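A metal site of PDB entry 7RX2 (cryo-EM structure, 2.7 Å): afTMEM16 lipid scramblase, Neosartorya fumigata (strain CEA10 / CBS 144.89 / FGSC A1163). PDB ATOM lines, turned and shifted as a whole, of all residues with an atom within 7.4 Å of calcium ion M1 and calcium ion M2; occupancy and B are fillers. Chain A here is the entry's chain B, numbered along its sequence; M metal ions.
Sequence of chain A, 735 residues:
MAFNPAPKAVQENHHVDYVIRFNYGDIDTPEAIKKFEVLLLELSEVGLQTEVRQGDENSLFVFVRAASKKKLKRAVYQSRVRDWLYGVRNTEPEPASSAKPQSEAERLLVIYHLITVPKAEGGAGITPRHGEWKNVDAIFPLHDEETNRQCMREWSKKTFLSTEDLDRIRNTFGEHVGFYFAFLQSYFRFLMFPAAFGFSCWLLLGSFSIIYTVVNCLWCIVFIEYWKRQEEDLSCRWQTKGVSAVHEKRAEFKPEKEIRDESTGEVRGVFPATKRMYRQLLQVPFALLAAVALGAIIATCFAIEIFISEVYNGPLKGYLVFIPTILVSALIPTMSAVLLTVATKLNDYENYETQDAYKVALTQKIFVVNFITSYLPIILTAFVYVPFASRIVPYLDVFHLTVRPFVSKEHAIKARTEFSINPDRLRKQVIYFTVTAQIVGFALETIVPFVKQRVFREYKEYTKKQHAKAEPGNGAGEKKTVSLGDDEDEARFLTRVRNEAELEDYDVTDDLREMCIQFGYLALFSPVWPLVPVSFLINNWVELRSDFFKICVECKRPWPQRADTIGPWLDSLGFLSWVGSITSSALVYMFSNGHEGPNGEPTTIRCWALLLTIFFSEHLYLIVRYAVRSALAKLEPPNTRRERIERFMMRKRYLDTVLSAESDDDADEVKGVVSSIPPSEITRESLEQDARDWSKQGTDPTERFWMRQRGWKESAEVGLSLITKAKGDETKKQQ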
ATOM      1  N   TYR A 180     -30.879   3.448   2.916  1.00  0.00           N
ATOM      2  CA  TYR A 180     -29.623   3.507   2.186  1.00  0.00           C
ATOM      3  C   TYR A 180     -29.761   2.915   0.790  1.00  0.00           C
ATOM      4  O   TYR A 180     -29.281   3.492  -0.178  1.00  0.00           O
ATOM      5  CB  TYR A 180     -28.521   2.796   2.959  1.00  0.00           C
ATOM      6  CG  TYR A 180     -27.327   2.449   2.112  1.00  0.00           C
ATOM      7  CD1 TYR A 180     -26.535   3.444   1.570  1.00  0.00           C
ATOM      8  CD2 TYR A 180     -27.014   1.142   1.829  1.00  0.00           C
ATOM      9  CE1 TYR A 180     -25.461   3.138   0.786  1.00  0.00           C
ATOM     10  CE2 TYR A 180     -25.936   0.828   1.043  1.00  0.00           C
ATOM     11  CZ  TYR A 180     -25.169   1.826   0.527  1.00  0.00           C
ATOM     12  OH  TYR A 180     -24.095   1.520  -0.256  1.00  0.00           O
ATOM     13  N   LEU A 184     -29.302   4.832  -2.632  1.00  0.00           N
ATOM     14  CA  LEU A 184     -28.309   4.386  -3.602  1.00  0.00           C
ATOM     15  C   LEU A 184     -28.936   4.072  -4.951  1.00  0.00           C
ATOM     16  O   LEU A 184     -28.334   4.347  -5.984  1.00  0.00           O
ATOM     17  CB  LEU A 184     -27.579   3.167  -3.064  1.00  0.00           C
ATOM     18  CG  LEU A 184     -26.509   2.570  -3.965  1.00  0.00           C
ATOM     19  CD1 LEU A 184     -25.522   3.641  -4.324  1.00  0.00           C
ATOM     20  CD2 LEU A 184     -25.826   1.438  -3.273  1.00  0.00           C
ATOM     21  N   ALA A 437      -9.564   4.080  -7.132  1.00  0.00           N
ATOM     22  CA  ALA A 437     -10.000   3.993  -5.748  1.00  0.00           C
ATOM     23  C   ALA A 437     -11.359   3.320  -5.609  1.00  0.00           C
ATOM     24  O   ALA A 437     -11.656   2.777  -4.549  1.00  0.00           O
ATOM     25  CB  ALA A 437     -10.052   5.384  -5.122  1.00  0.00           C
ATOM     26  N   GLN A 438     -12.183   3.344  -6.658  1.00  0.00           N
ATOM     27  CA  GLN A 438     -13.424   2.590  -6.607  1.00  0.00           C
ATOM     28  C   GLN A 438     -13.205   1.114  -6.874  1.00  0.00           C
ATOM     29  O   GLN A 438     -13.939   0.271  -6.340  1.00  0.00           O
ATOM     30  CB  GLN A 438     -14.436   3.157  -7.611  1.00  0.00           C
ATOM     31  CG  GLN A 438     -14.543   4.672  -7.618  1.00  0.00           C
ATOM     32  CD  GLN A 438     -15.035   5.233  -6.305  1.00  0.00           C
ATOM     33  OE1 GLN A 438     -14.383   6.075  -5.704  1.00  0.00           O
ATOM     34  NE2 GLN A 438     -16.197   4.779  -5.866  1.00  0.00           N
ATOM     35  N   ILE A 439     -12.199   0.775  -7.678  1.00  0.00           N
ATOM     36  CA  ILE A 439     -11.875  -0.628  -7.930  1.00  0.00           C
ATOM     37  C   ILE A 439     -11.092  -1.208  -6.769  1.00  0.00           C
ATOM     38  O   ILE A 439     -11.390  -2.306  -6.284  1.00  0.00           O
ATOM     39  CB  ILE A 439     -11.109  -0.763  -9.261  1.00  0.00           C
ATOM     40  CG1 ILE A 439     -11.951  -0.192 -10.401  1.00  0.00           C
ATOM     41  CG2 ILE A 439     -10.754  -2.206  -9.524  1.00  0.00           C
ATOM     42  CD1 ILE A 439     -11.367  -0.437 -11.762  1.00  0.00           C
ATOM     43  N   VAL A 440     -10.085  -0.485  -6.286  1.00  0.00           N
ATOM     44  CA  VAL A 440      -9.330  -0.960  -5.132  1.00  0.00           C
ATOM     45  C   VAL A 440     -10.216  -1.014  -3.899  1.00  0.00           C
ATOM     46  O   VAL A 440     -10.181  -1.987  -3.134  1.00  0.00           O
ATOM     47  CB  VAL A 440      -8.102  -0.065  -4.882  1.00  0.00           C
ATOM     48  CG1 VAL A 440      -7.633  -0.222  -3.448  1.00  0.00           C
ATOM     49  CG2 VAL A 440      -6.989  -0.414  -5.856  1.00  0.00           C
ATOM     50  N   GLY A 441     -11.028   0.016  -3.683  1.00  0.00           N
ATOM     51  CA  GLY A 441     -11.910   0.036  -2.527  1.00  0.00           C
ATOM     52  C   GLY A 441     -12.946  -1.058  -2.525  1.00  0.00           C
ATOM     53  O   GLY A 441     -13.351  -1.508  -1.439  1.00  0.00           O
ATOM     54  N   PHE A 442     -13.385  -1.503  -3.693  1.00  0.00           N
ATOM     55  CA  PHE A 442     -14.287  -2.652  -3.765  1.00  0.00           C
ATOM     56  C   PHE A 442     -13.637  -3.912  -3.206  1.00  0.00           C
ATOM     57  O   PHE A 442     -14.327  -4.758  -2.640  1.00  0.00           O
ATOM     58  CB  PHE A 442     -14.727  -2.868  -5.204  1.00  0.00           C
ATOM     59  CG  PHE A 442     -15.310  -4.219  -5.460  1.00  0.00           C
ATOM     60  CD1 PHE A 442     -16.606  -4.513  -5.090  1.00  0.00           C
ATOM     61  CD2 PHE A 442     -14.559  -5.185  -6.101  1.00  0.00           C
ATOM     62  CE1 PHE A 442     -17.134  -5.753  -5.334  1.00  0.00           C
ATOM     63  CE2 PHE A 442     -15.091  -6.439  -6.344  1.00  0.00           C
ATOM     64  CZ  PHE A 442     -16.377  -6.721  -5.967  1.00  0.00           C
ATOM     65  N   ALA A 443     -12.315  -4.036  -3.350  1.00  0.00           N
ATOM     66  CA  ALA A 443     -11.603  -5.210  -2.866  1.00  0.00           C
ATOM     67  C   ALA A 443     -11.474  -5.228  -1.357  1.00  0.00           C
ATOM     68  O   ALA A 443     -11.738  -6.249  -0.722  1.00  0.00           O
ATOM     69  CB  ALA A 443     -10.221  -5.294  -3.520  1.00  0.00           C
ATOM     70  N   GLU A 445     -13.361  -3.741   0.696  1.00  0.00           N
ATOM     71  CA  GLU A 445     -14.667  -3.608   1.333  1.00  0.00           C
ATOM     72  C   GLU A 445     -15.419  -4.924   1.401  1.00  0.00           C
ATOM     73  O   GLU A 445     -16.050  -5.220   2.427  1.00  0.00           O
ATOM     74  CB  GLU A 445     -15.507  -2.575   0.573  1.00  0.00           C
ATOM     75  CG  GLU A 445     -16.848  -2.275   1.212  1.00  0.00           C
ATOM     76  CD  GLU A 445     -17.614  -1.221   0.446  1.00  0.00           C
ATOM     77  OE1 GLU A 445     -17.052  -0.676  -0.527  1.00  0.00           O
ATOM     78  OE2 GLU A 445     -18.774  -0.956   0.809  1.00  0.00           O
ATOM     79  N   THR A 446     -15.366  -5.737   0.350  1.00  0.00           N
ATOM     80  CA  THR A 446     -16.190  -6.946   0.285  1.00  0.00           C
ATOM     81  C   THR A 446     -15.387  -8.221   0.110  1.00  0.00           C
ATOM     82  O   THR A 446     -15.800  -9.276   0.597  1.00  0.00           O
ATOM     83  CB  THR A 446     -17.200  -6.822  -0.854  1.00  0.00           C
ATOM     84  OG1 THR A 446     -17.812  -5.527  -0.802  1.00  0.00           O
ATOM     85  CG2 THR A 446     -18.275  -7.886  -0.721  1.00  0.00           C
ATOM     86  N   TYR A 506     -22.246  -4.735  11.115  1.00  0.00           N
ATOM     87  CA  TYR A 506     -22.577  -3.821   9.996  1.00  0.00           C
ATOM     88  C   TYR A 506     -23.051  -2.460  10.520  1.00  0.00           C
ATOM     89  O   TYR A 506     -23.825  -2.391  11.500  1.00  0.00           O
ATOM     90  CB  TYR A 506     -23.666  -4.443   9.115  1.00  0.00           C
ATOM     91  CG  TYR A 506     -24.067  -3.595   7.938  1.00  0.00           C
ATOM     92  CD1 TYR A 506     -23.267  -3.514   6.816  1.00  0.00           C
ATOM     93  CD2 TYR A 506     -25.228  -2.840   7.963  1.00  0.00           C
ATOM     94  CE1 TYR A 506     -23.616  -2.732   5.730  1.00  0.00           C
ATOM     95  CE2 TYR A 506     -25.593  -2.046   6.887  1.00  0.00           C
ATOM     96  CZ  TYR A 506     -24.780  -1.983   5.768  1.00  0.00           C
ATOM     97  OH  TYR A 506     -25.135  -1.213   4.708  1.00  0.00           O
ATOM     98  N   ASP A 510     -21.222   3.727   7.330  1.00  0.00           N
ATOM     99  CA  ASP A 510     -19.959   3.537   6.573  1.00  0.00           C
ATOM    100  C   ASP A 510     -20.297   3.544   5.071  1.00  0.00           C
ATOM    101  O   ASP A 510     -19.527   4.132   4.294  1.00  0.00           O
ATOM    102  CB  ASP A 510     -19.245   2.244   6.975  1.00  0.00           C
ATOM    103  CG  ASP A 510     -18.846   2.207   8.438  1.00  0.00           C
ATOM    104  OD1 ASP A 510     -18.977   3.241   9.113  1.00  0.00           O
ATOM    105  OD2 ASP A 510     -18.393   1.130   8.886  1.00  0.00           O
ATOM    106  N   ASP A 511     -21.417   2.903   4.709  1.00  0.00           N
ATOM    107  CA  ASP A 511     -21.866   2.825   3.288  1.00  0.00           C
ATOM    108  C   ASP A 511     -22.346   4.198   2.837  1.00  0.00           C
ATOM    109  O   ASP A 511     -21.952   4.627   1.732  1.00  0.00           O
ATOM    110  CB  ASP A 511     -22.940   1.755   3.105  1.00  0.00           C
ATOM    111  CG  ASP A 511     -22.371   0.355   2.976  1.00  0.00           C
ATOM    112  OD1 ASP A 511     -21.228   0.226   2.494  1.00  0.00           O
ATOM    113  OD2 ASP A 511     -23.061  -0.602   3.368  1.00  0.00           O
ATOM    114  N   LEU A 512     -23.180   4.871   3.640  1.00  0.00           N
ATOM    115  CA  LEU A 512     -23.665   6.196   3.292  1.00  0.00           C
ATOM    116  C   LEU A 512     -22.529   7.182   3.162  1.00  0.00           C
ATOM    117  O   LEU A 512     -22.568   8.052   2.297  1.00  0.00           O
ATOM    118  CB  LEU A 512     -24.653   6.684   4.344  1.00  0.00           C
ATOM    119  CG  LEU A 512     -26.087   6.187   4.206  1.00  0.00           C
ATOM    120  CD1 LEU A 512     -26.860   6.480   5.462  1.00  0.00           C
ATOM    121  CD2 LEU A 512     -26.737   6.821   3.017  1.00  0.00           C
ATOM    122  N   GLU A 514     -19.459   6.543   2.177  1.00  0.00           N
ATOM    123  CA  GLU A 514     -18.723   6.279   0.956  1.00  0.00           C
ATOM    124  C   GLU A 514     -19.469   6.783  -0.270  1.00  0.00           C
ATOM    125  O   GLU A 514     -18.830   7.200  -1.241  1.00  0.00           O
ATOM    126  CB  GLU A 514     -18.448   4.792   0.854  1.00  0.00           C
ATOM    127  CG  GLU A 514     -17.815   4.369  -0.425  1.00  0.00           C
ATOM    128  CD  GLU A 514     -17.839   2.871  -0.596  1.00  0.00           C
ATOM    129  OE1 GLU A 514     -17.035   2.342  -1.391  1.00  0.00           O
ATOM    130  OE2 GLU A 514     -18.671   2.226   0.073  1.00  0.00           O
ATOM    131  N   MET A 515     -20.799   6.742  -0.253  1.00  0.00           N
ATOM    132  CA  MET A 515     -21.565   7.222  -1.399  1.00  0.00           C
ATOM    133  C   MET A 515     -21.587   8.744  -1.455  1.00  0.00           C
ATOM    134  O   MET A 515     -21.580   9.321  -2.538  1.00  0.00           O
ATOM    135  CB  MET A 515     -22.986   6.678  -1.351  1.00  0.00           C
ATOM    136  CG  MET A 515     -23.144   5.302  -1.944  1.00  0.00           C
ATOM    137  SD  MET A 515     -22.367   5.110  -3.556  1.00  0.00           S
ATOM    138  CE  MET A 515     -20.916   4.174  -3.128  1.00  0.00           C
ATOM    139  N   GLN A 518     -18.226   9.957  -2.548  1.00  0.00           N
ATOM    140  CA  GLN A 518     -18.152   9.763  -3.987  1.00  0.00           C
ATOM    141  C   GLN A 518     -18.919  10.843  -4.727  1.00  0.00           C
ATOM    142  O   GLN A 518     -18.488  11.285  -5.795  1.00  0.00           O
ATOM    143  CB  GLN A 518     -18.671   8.376  -4.355  1.00  0.00           C
ATOM    144  CG  GLN A 518     -18.611   8.089  -5.806  1.00  0.00           C
ATOM    145  CD  GLN A 518     -19.586   7.042  -6.233  1.00  0.00           C
ATOM    146  OE1 GLN A 518     -20.744   7.340  -6.498  1.00  0.00           O
ATOM    147  NE2 GLN A 518     -19.141   5.810  -6.308  1.00  0.00           N
ATOM    148  N   ASN A 539     -19.923   1.778 -11.174  1.00  0.00           N
ATOM    149  CA  ASN A 539     -19.565   1.365  -9.826  1.00  0.00           C
ATOM    150  C   ASN A 539     -20.793   1.199  -8.949  1.00  0.00           C
ATOM    151  O   ASN A 539     -20.878   0.257  -8.156  1.00  0.00           O
ATOM    152  CB  ASN A 539     -18.605   2.375  -9.207  1.00  0.00           C
ATOM    153  CG  ASN A 539     -18.270   2.050  -7.779  1.00  0.00           C
ATOM    154  OD1 ASN A 539     -17.363   1.272  -7.515  1.00  0.00           O
ATOM    155  ND2 ASN A 539     -19.000   2.643  -6.847  1.00  0.00           N
ATOM    156  N   ASN A 540     -21.752   2.110  -9.065  1.00  0.00           N
ATOM    157  CA  ASN A 540     -22.889   2.089  -8.168  1.00  0.00           C
ATOM    158  C   ASN A 540     -23.853   0.954  -8.458  1.00  0.00           C
ATOM    159  O   ASN A 540     -24.582   0.543  -7.550  1.00  0.00           O
ATOM    160  CB  ASN A 540     -23.627   3.421  -8.214  1.00  0.00           C
ATOM    161  CG  ASN A 540     -22.881   4.511  -7.495  1.00  0.00           C
ATOM    162  OD1 ASN A 540     -21.826   4.279  -6.918  1.00  0.00           O
ATOM    163  ND2 ASN A 540     -23.426   5.718  -7.538  1.00  0.00           N
ATOM    164  N   VAL A 542     -22.788  -2.136  -9.319  1.00  0.00           N
ATOM    165  CA  VAL A 542     -22.111  -3.196  -8.581  1.00  0.00           C
ATOM    166  C   VAL A 542     -22.195  -2.957  -7.086  1.00  0.00           C
ATOM    167  O   VAL A 542     -22.365  -3.905  -6.314  1.00  0.00           O
ATOM    168  CB  VAL A 542     -20.644  -3.302  -9.032  1.00  0.00           C
ATOM    169  CG1 VAL A 542     -19.952  -4.386  -8.271  1.00  0.00           C
ATOM    170  CG2 VAL A 542     -20.563  -3.546 -10.515  1.00  0.00           C
ATOM    171  N   GLU A 543     -22.077  -1.702  -6.655  1.00  0.00           N
ATOM    172  CA  GLU A 543     -22.057  -1.397  -5.227  1.00  0.00           C
ATOM    173  C   GLU A 543     -23.338  -1.838  -4.541  1.00  0.00           C
ATOM    174  O   GLU A 543     -23.317  -2.308  -3.406  1.00  0.00           O
ATOM    175  CB  GLU A 543     -21.827   0.094  -5.016  1.00  0.00           C
ATOM    176  CG  GLU A 543     -21.644   0.485  -3.572  1.00  0.00           C
ATOM    177  CD  GLU A 543     -20.200   0.476  -3.171  1.00  0.00           C
ATOM    178  OE1 GLU A 543     -19.355   0.444  -4.072  1.00  0.00           O
ATOM    179  OE2 GLU A 543     -19.908   0.493  -1.965  1.00  0.00           O
ATOM    180  N   LEU A 544     -24.467  -1.681  -5.220  1.00  0.00           N
ATOM    181  CA  LEU A 544     -25.727  -2.101  -4.639  1.00  0.00           C
ATOM    182  C   LEU A 544     -25.798  -3.599  -4.466  1.00  0.00           C
ATOM    183  O   LEU A 544     -26.415  -4.092  -3.514  1.00  0.00           O
ATOM    184  CB  LEU A 544     -26.875  -1.592  -5.508  1.00  0.00           C
ATOM    185  CG  LEU A 544     -28.246  -1.594  -4.856  1.00  0.00           C
ATOM    186  CD1 LEU A 544     -29.069  -0.499  -5.444  1.00  0.00           C
ATOM    187  CD2 LEU A 544     -28.907  -2.947  -5.066  1.00  0.00           C
ATOM    188  N   SER A 546     -22.995  -5.698  -4.167  1.00  0.00           N
ATOM    189  CA  SER A 546     -21.969  -6.134  -3.230  1.00  0.00           C
ATOM    190  C   SER A 546     -22.184  -5.589  -1.826  1.00  0.00           C
ATOM    191  O   SER A 546     -21.692  -6.188  -0.867  1.00  0.00           O
ATOM    192  CB  SER A 546     -20.589  -5.714  -3.731  1.00  0.00           C
ATOM    193  OG  SER A 546     -20.356  -4.347  -3.487  1.00  0.00           O
ATOM    194  N   ASP A 547     -22.901  -4.476  -1.671  1.00  0.00           N
ATOM    195  CA  ASP A 547     -23.265  -4.026  -0.339  1.00  0.00           C
ATOM    196  C   ASP A 547     -24.354  -4.903   0.262  1.00  0.00           C
ATOM    197  O   ASP A 547     -24.367  -5.119   1.476  1.00  0.00           O
ATOM    198  CB  ASP A 547     -23.728  -2.575  -0.362  1.00  0.00           C
ATOM    199  CG  ASP A 547     -22.590  -1.612  -0.156  1.00  0.00           C
ATOM    200  OD1 ASP A 547     -21.469  -2.043   0.153  1.00  0.00           O
ATOM    201  OD2 ASP A 547     -22.820  -0.392  -0.316  1.00  0.00           O
ATOM    202  N   LYS A 550     -22.546  -8.058   1.231  1.00  0.00           N
ATOM    203  CA  LYS A 550     -21.771  -7.852   2.446  1.00  0.00           C
ATOM    204  C   LYS A 550     -22.630  -7.934   3.696  1.00  0.00           C
ATOM    205  O   LYS A 550     -22.164  -8.413   4.740  1.00  0.00           O
ATOM    206  CB  LYS A 550     -21.064  -6.500   2.384  1.00  0.00           C
ATOM    207  CG  LYS A 550     -20.731  -5.934   3.731  1.00  0.00           C
ATOM    208  CD  LYS A 550     -19.626  -4.919   3.647  1.00  0.00           C
ATOM    209  CE  LYS A 550     -20.055  -3.708   2.870  1.00  0.00           C
ATOM    210  NZ  LYS A 550     -20.956  -2.840   3.649  1.00  0.00           N
HETATM  211 CA    CA M   1     -17.285   0.459  -2.840  1.00  0.00          CA
HETATM  212 CA    CA M   2     -20.487   0.623   0.375  1.00  0.00          CA
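OD2 of Asp 511 is in salt-bridge range of NZ of Lys 550 (3.1 Å). The side-chain carboxylate of Asp 511 is in hydrogen-bond range of the side-chain hydroxyl of Tyr 506 (2.5 Å). OD1 of Asp 547 lies close to NZ of Lys 550, at 3.6 Å.
The nearest printed residue that does not touch calcium ion M1 is Phe 442 (4.4 Å).
Residues that only touch calcium ion M2: Tyr 180. Six residues have an atom within 4 Å of calcium ion M2: Tyr 180, Glu 445, Asp 511, Glu 514, Glu 543 and Asp 547. The nearest printed residue that does not touch calcium ion M2 is Lys 550 (4.8 Å).
Calcium ion M1 is bound by OE1 of Glu 514 (2.4 Å), OE1 of Glu 543 (2.4 Å), OE1 of Glu 445 (2.6 Å) and OE2 of Glu 543 (2.8 Å).
OD1 of Asp 511 is bound to calcium ion M2, at 2.3 Å. OE2 of Glu 445 is bound to calcium ion M2 (2.4 Å). The side-chain carboxylate (OE2) of Glu 543 binds calcium ion M2, at 2.4 Å. The side-chain carboxylate (OE2) of Glu 514 is bound to calcium ion M2 (2.4 Å). Calcium ion M2 is bound by OD2 of Asp 547, at 2.6 Å. OD1 of Asp 547 is bound to calcium ion M2 (2.8 Å). Calcium ion M2 has six donor atoms within binding distance.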
